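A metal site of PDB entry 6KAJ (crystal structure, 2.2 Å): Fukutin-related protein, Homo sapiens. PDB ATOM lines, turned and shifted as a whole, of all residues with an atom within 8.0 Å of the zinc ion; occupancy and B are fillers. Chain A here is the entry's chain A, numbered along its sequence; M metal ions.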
ATOM      1  N   ARG A 235     -11.898 -24.311 -11.391  1.00  0.00           N
ATOM      2  CA  ARG A 235     -10.975 -24.980 -12.304  1.00  0.00           C
ATOM      3  C   ARG A 235     -11.421 -26.369 -12.706  1.00  0.00           C
ATOM      4  O   ARG A 235     -10.950 -26.900 -13.715  1.00  0.00           O
ATOM      5  CB  ARG A 235      -9.588 -25.082 -11.655  1.00  0.00           C
ATOM      6  CG  ARG A 235      -8.882 -23.762 -11.469  1.00  0.00           C
ATOM      7  CD  ARG A 235      -8.271 -23.261 -12.772  1.00  0.00           C
ATOM      8  NE  ARG A 235      -7.319 -22.194 -12.519  1.00  0.00           N
ATOM      9  CZ  ARG A 235      -7.649 -20.925 -12.332  1.00  0.00           C
ATOM     10  NH1 ARG A 235      -8.922 -20.556 -12.406  1.00  0.00           N
ATOM     11  NH2 ARG A 235      -6.719 -20.018 -12.073  1.00  0.00           N
ATOM     12  N   TRP A 246     -12.421 -29.805 -17.090  1.00  0.00           N
ATOM     13  CA  TRP A 246     -11.305 -28.962 -16.672  1.00  0.00           C
ATOM     14  C   TRP A 246     -11.394 -27.582 -17.298  1.00  0.00           C
ATOM     15  O   TRP A 246     -11.790 -27.433 -18.458  1.00  0.00           O
ATOM     16  CB  TRP A 246      -9.953 -29.600 -17.046  1.00  0.00           C
ATOM     17  CG  TRP A 246      -9.685 -30.874 -16.312  1.00  0.00           C
ATOM     18  CD1 TRP A 246      -9.907 -32.139 -16.773  1.00  0.00           C
ATOM     19  CD2 TRP A 246      -9.144 -31.013 -14.992  1.00  0.00           C
ATOM     20  NE1 TRP A 246      -9.537 -33.058 -15.824  1.00  0.00           N
ATOM     21  CE2 TRP A 246      -9.065 -32.397 -14.720  1.00  0.00           C
ATOM     22  CE3 TRP A 246      -8.721 -30.106 -14.021  1.00  0.00           C
ATOM     23  CZ2 TRP A 246      -8.566 -32.888 -13.507  1.00  0.00           C
ATOM     24  CZ3 TRP A 246      -8.231 -30.600 -12.818  1.00  0.00           C
ATOM     25  CH2 TRP A 246      -8.160 -31.978 -12.578  1.00  0.00           C
ATOM     26  N   PHE A 247     -11.018 -26.569 -16.520  1.00  0.00           N
ATOM     27  CA  PHE A 247     -11.017 -25.181 -16.964  1.00  0.00           C
ATOM     28  C   PHE A 247      -9.765 -24.452 -16.471  1.00  0.00           C
ATOM     29  O   PHE A 247      -9.805 -23.232 -16.254  1.00  0.00           O
ATOM     30  CB  PHE A 247     -12.283 -24.463 -16.512  1.00  0.00           C
ATOM     31  CG  PHE A 247     -13.547 -25.086 -17.053  1.00  0.00           C
ATOM     32  CD1 PHE A 247     -14.050 -24.691 -18.282  1.00  0.00           C
ATOM     33  CD2 PHE A 247     -14.191 -26.106 -16.370  1.00  0.00           C
ATOM     34  CE1 PHE A 247     -15.192 -25.270 -18.799  1.00  0.00           C
ATOM     35  CE2 PHE A 247     -15.332 -26.695 -16.877  1.00  0.00           C
ATOM     36  CZ  PHE A 247     -15.834 -26.268 -18.097  1.00  0.00           C
ATOM     37  N   GLY A 248      -8.663 -25.175 -16.287  1.00  0.00           N
ATOM     38  CA  GLY A 248      -7.421 -24.587 -15.848  1.00  0.00           C
ATOM     39  C   GLY A 248      -6.280 -24.735 -16.854  1.00  0.00           C
ATOM     40  O   GLY A 248      -6.491 -24.596 -18.061  1.00  0.00           O
ATOM     41  N   CYS A 249      -5.086 -25.033 -16.350  1.00  0.00           N
ATOM     42  CA  CYS A 249      -3.902 -25.184 -17.179  1.00  0.00           C
ATOM     43  C   CYS A 249      -3.801 -26.615 -17.729  1.00  0.00           C
ATOM     44  O   CYS A 249      -4.537 -27.518 -17.327  1.00  0.00           O
ATOM     45  CB  CYS A 249      -2.652 -24.831 -16.371  1.00  0.00           C
ATOM     46  SG  CYS A 249      -2.278 -26.006 -15.054  1.00  0.00           S
ATOM     47  N   ASN A 250      -2.878 -26.800 -18.660  1.00  0.00           N
ATOM     48  CA  ASN A 250      -2.634 -28.117 -19.260  1.00  0.00           C
ATOM     49  C   ASN A 250      -1.252 -28.102 -19.931  1.00  0.00           C
ATOM     50  O   ASN A 250      -0.451 -27.191 -19.729  1.00  0.00           O
ATOM     51  CB  ASN A 250      -3.733 -28.491 -20.258  1.00  0.00           C
ATOM     52  CG  ASN A 250      -3.860 -27.498 -21.402  1.00  0.00           C
ATOM     53  OD1 ASN A 250      -2.896 -27.251 -22.131  1.00  0.00           O
ATOM     54  ND2 ASN A 250      -5.049 -26.930 -21.568  1.00  0.00           N
ATOM     55  N   THR A 253      -0.522 -24.803 -22.087  1.00  0.00           N
ATOM     56  CA  THR A 253      -0.641 -23.469 -21.533  1.00  0.00           C
ATOM     57  C   THR A 253       0.457 -23.217 -20.518  1.00  0.00           C
ATOM     58  O   THR A 253       1.231 -24.110 -20.165  1.00  0.00           O
ATOM     59  CB  THR A 253      -2.023 -23.270 -20.895  1.00  0.00           C
ATOM     60  OG1 THR A 253      -2.048 -23.895 -19.610  1.00  0.00           O
ATOM     61  CG2 THR A 253      -3.108 -23.868 -21.778  1.00  0.00           C
ATOM     62  N   THR A 254       0.516 -21.971 -20.047  1.00  0.00           N
ATOM     63  CA  THR A 254       1.286 -21.701 -18.842  1.00  0.00           C
ATOM     64  C   THR A 254       0.579 -22.340 -17.654  1.00  0.00           C
ATOM     65  O   THR A 254      -0.578 -22.771 -17.738  1.00  0.00           O
ATOM     66  CB  THR A 254       1.442 -20.195 -18.626  1.00  0.00           C
ATOM     67  OG1 THR A 254       0.167 -19.625 -18.308  1.00  0.00           O
ATOM     68  CG2 THR A 254       1.982 -19.530 -19.868  1.00  0.00           C
ATOM     69  N   ARG A 255       1.278 -22.405 -16.520  1.00  0.00           N
ATOM     70  CA  ARG A 255       0.594 -22.861 -15.320  1.00  0.00           C
ATOM     71  C   ARG A 255      -0.291 -21.730 -14.782  1.00  0.00           C
ATOM     72  O   ARG A 255      -0.215 -20.582 -15.232  1.00  0.00           O
ATOM     73  CB  ARG A 255       1.602 -23.322 -14.265  1.00  0.00           C
ATOM     74  CG  ARG A 255       2.420 -22.206 -13.678  1.00  0.00           C
ATOM     75  CD  ARG A 255       3.507 -22.744 -12.780  1.00  0.00           C
ATOM     76  NE  ARG A 255       4.075 -21.690 -11.950  1.00  0.00           N
ATOM     77  CZ  ARG A 255       5.247 -21.787 -11.339  1.00  0.00           C
ATOM     78  NH1 ARG A 255       5.983 -22.887 -11.463  1.00  0.00           N
ATOM     79  NH2 ARG A 255       5.689 -20.773 -10.603  1.00  0.00           N
ATOM     80  N   CYS A 256      -1.141 -22.082 -13.811  1.00  0.00           N
ATOM     81  CA  CYS A 256      -2.157 -21.127 -13.370  1.00  0.00           C
ATOM     82  C   CYS A 256      -1.549 -19.956 -12.613  1.00  0.00           C
ATOM     83  O   CYS A 256      -2.058 -18.839 -12.702  1.00  0.00           O
ATOM     84  CB  CYS A 256      -3.213 -21.832 -12.527  1.00  0.00           C
ATOM     85  SG  CYS A 256      -4.204 -23.003 -13.475  1.00  0.00           S
ATOM     86  N   PHE A 257      -0.486 -20.181 -11.857  1.00  0.00           N
ATOM     87  CA  PHE A 257       0.105 -19.132 -11.033  1.00  0.00           C
ATOM     88  C   PHE A 257       1.457 -18.731 -11.589  1.00  0.00           C
ATOM     89  O   PHE A 257       2.228 -19.574 -12.057  1.00  0.00           O
ATOM     90  CB  PHE A 257       0.225 -19.559  -9.559  1.00  0.00           C
ATOM     91  CG  PHE A 257       0.881 -20.897  -9.347  1.00  0.00           C
ATOM     92  CD1 PHE A 257       0.181 -22.074  -9.561  1.00  0.00           C
ATOM     93  CD2 PHE A 257       2.202 -20.973  -8.910  1.00  0.00           C
ATOM     94  CE1 PHE A 257       0.792 -23.311  -9.360  1.00  0.00           C
ATOM     95  CE2 PHE A 257       2.808 -22.200  -8.700  1.00  0.00           C
ATOM     96  CZ  PHE A 257       2.109 -23.368  -8.935  1.00  0.00           C
ATOM     97  N   THR A 274      -3.720 -24.855  -4.005  1.00  0.00           N
ATOM     98  CA  THR A 274      -3.213 -25.057  -5.352  1.00  0.00           C
ATOM     99  C   THR A 274      -4.365 -25.408  -6.298  1.00  0.00           C
ATOM    100  O   THR A 274      -5.255 -26.187  -5.923  1.00  0.00           O
ATOM    101  CB  THR A 274      -2.165 -26.154  -5.386  1.00  0.00           C
ATOM    102  OG1 THR A 274      -1.153 -25.884  -4.392  1.00  0.00           O
ATOM    103  CG2 THR A 274      -1.499 -26.235  -6.760  1.00  0.00           C
ATOM    104  N   PRO A 275      -4.406 -24.844  -7.497  1.00  0.00           N
ATOM    105  CA  PRO A 275      -5.409 -25.234  -8.482  1.00  0.00           C
ATOM    106  C   PRO A 275      -5.356 -26.724  -8.743  1.00  0.00           C
ATOM    107  O   PRO A 275      -4.269 -27.317  -8.811  1.00  0.00           O
ATOM    108  CB  PRO A 275      -5.019 -24.431  -9.721  1.00  0.00           C
ATOM    109  CG  PRO A 275      -4.437 -23.167  -9.133  1.00  0.00           C
ATOM    110  CD  PRO A 275      -3.678 -23.624  -7.918  1.00  0.00           C
ATOM    111  N   PRO A 276      -6.520 -27.379  -8.896  1.00  0.00           N
ATOM    112  CA  PRO A 276      -6.516 -28.825  -9.104  1.00  0.00           C
ATOM    113  C   PRO A 276      -5.914 -29.239 -10.437  1.00  0.00           C
ATOM    114  O   PRO A 276      -5.391 -30.352 -10.568  1.00  0.00           O
ATOM    115  CB  PRO A 276      -8.002 -29.196  -8.992  1.00  0.00           C
ATOM    116  CG  PRO A 276      -8.725 -27.954  -9.399  1.00  0.00           C
ATOM    117  CD  PRO A 276      -7.874 -26.816  -8.880  1.00  0.00           C
ATOM    118  N   CYS A 277      -5.994 -28.367 -11.447  1.00  0.00           N
ATOM    119  CA  CYS A 277      -5.258 -28.616 -12.691  1.00  0.00           C
ATOM    120  C   CYS A 277      -3.757 -28.622 -12.437  1.00  0.00           C
ATOM    121  O   CYS A 277      -3.032 -29.444 -13.003  1.00  0.00           O
ATOM    122  CB  CYS A 277      -5.635 -27.551 -13.720  1.00  0.00           C
ATOM    123  SG  CYS A 277      -5.509 -25.887 -13.053  1.00  0.00           S
ATOM    124  N   CYS A 278      -3.276 -27.731 -11.568  1.00  0.00           N
ATOM    125  CA  CYS A 278      -1.841 -27.708 -11.263  1.00  0.00           C
ATOM    126  C   CYS A 278      -1.423 -28.940 -10.482  1.00  0.00           C
ATOM    127  O   CYS A 278      -0.355 -29.503 -10.726  1.00  0.00           O
ATOM    128  CB  CYS A 278      -1.503 -26.427 -10.496  1.00  0.00           C
ATOM    129  SG  CYS A 278      -1.708 -24.898 -11.449  1.00  0.00           S
ATOM    130  N   LEU A 279      -2.243 -29.368  -9.513  1.00  0.00           N
ATOM    131  CA  LEU A 279      -1.927 -30.589  -8.775  1.00  0.00           C
ATOM    132  C   LEU A 279      -1.912 -31.797  -9.713  1.00  0.00           C
ATOM    133  O   LEU A 279      -1.035 -32.655  -9.612  1.00  0.00           O
ATOM    134  CB  LEU A 279      -2.927 -30.798  -7.640  1.00  0.00           C
ATOM    135  CG  LEU A 279      -2.850 -29.805  -6.475  1.00  0.00           C
ATOM    136  CD1 LEU A 279      -4.022 -30.000  -5.504  1.00  0.00           C
ATOM    137  CD2 LEU A 279      -1.528 -29.936  -5.732  1.00  0.00           C
ATOM    138  N   ARG A 280      -2.883 -31.862 -10.622  1.00  0.00           N
ATOM    139  CA  ARG A 280      -2.937 -32.946 -11.597  1.00  0.00           C
ATOM    140  C   ARG A 280      -1.660 -33.022 -12.418  1.00  0.00           C
ATOM    141  O   ARG A 280      -1.079 -34.103 -12.594  1.00  0.00           O
ATOM    142  CB  ARG A 280      -4.156 -32.783 -12.501  1.00  0.00           C
ATOM    143  CG  ARG A 280      -4.469 -33.986 -13.391  1.00  0.00           C
ATOM    144  CD  ARG A 280      -5.139 -33.533 -14.664  1.00  0.00           C
ATOM    145  NE  ARG A 280      -4.292 -32.591 -15.397  1.00  0.00           N
ATOM    146  CZ  ARG A 280      -3.250 -32.947 -16.152  1.00  0.00           C
ATOM    147  NH1 ARG A 280      -2.932 -34.235 -16.289  1.00  0.00           N
ATOM    148  NH2 ARG A 280      -2.539 -32.017 -16.760  1.00  0.00           N
ATOM    149  N   ALA A 281      -1.178 -31.869 -12.897  1.00  0.00           N
ATOM    150  CA  ALA A 281       0.037 -31.866 -13.710  1.00  0.00           C
ATOM    151  C   ALA A 281       1.256 -32.275 -12.893  1.00  0.00           C
ATOM    152  O   ALA A 281       2.161 -32.925 -13.426  1.00  0.00           O
ATOM    153  CB  ALA A 281       0.248 -30.484 -14.338  1.00  0.00           C
ATOM    154  N   ASN A 371       4.339 -25.098 -19.647  1.00  0.00           N
ATOM    155  CA  ASN A 371       3.772 -25.264 -18.306  1.00  0.00           C
ATOM    156  C   ASN A 371       4.898 -25.662 -17.341  1.00  0.00           C
ATOM    157  O   ASN A 371       5.321 -26.817 -17.320  1.00  0.00           O
ATOM    158  CB  ASN A 371       2.658 -26.298 -18.309  1.00  0.00           C
ATOM    159  CG  ASN A 371       1.847 -26.301 -17.020  1.00  0.00           C
ATOM    160  OD1 ASN A 371       2.403 -26.199 -15.924  1.00  0.00           O
ATOM    161  ND2 ASN A 371       0.527 -26.404 -17.144  1.00  0.00           N
ATOM    162  N   LEU A 373       5.197 -26.146 -14.113  1.00  0.00           N
ATOM    163  CA  LEU A 373       5.110 -27.004 -12.944  1.00  0.00           C
ATOM    164  C   LEU A 373       6.157 -28.099 -13.069  1.00  0.00           C
ATOM    165  O   LEU A 373       6.432 -28.594 -14.166  1.00  0.00           O
ATOM    166  CB  LEU A 373       3.705 -27.603 -12.838  1.00  0.00           C
ATOM    167  CG  LEU A 373       2.604 -26.585 -12.604  1.00  0.00           C
ATOM    168  CD1 LEU A 373       1.248 -27.155 -12.998  1.00  0.00           C
ATOM    169  CD2 LEU A 373       2.594 -26.146 -11.146  1.00  0.00           C
HETATM  170 ZN    ZN M   1      -3.313 -25.149 -13.126  1.00  0.00          ZN
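SG of Cys 249 sits close to ND2 of Asn 371. SG of Cys 256 lies close to NE of Arg 235.
Merely in contact with the zinc ion: Pro 275. Five residues have an atom within 4 Å of the zinc ion: Cys 249, Cys 256, Pro 275, Cys 277 and Cys 278. The nearest printed residue that does not touch the zinc ion is Gly 248 (4.8 Å).
The zinc ion is bound by SG of Cys 277 (2.3 Å), SG of Cys 278 (2.3 Å), SG of Cys 249 (2.4 Å) and SG of Cys 256 (2.3 Å).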
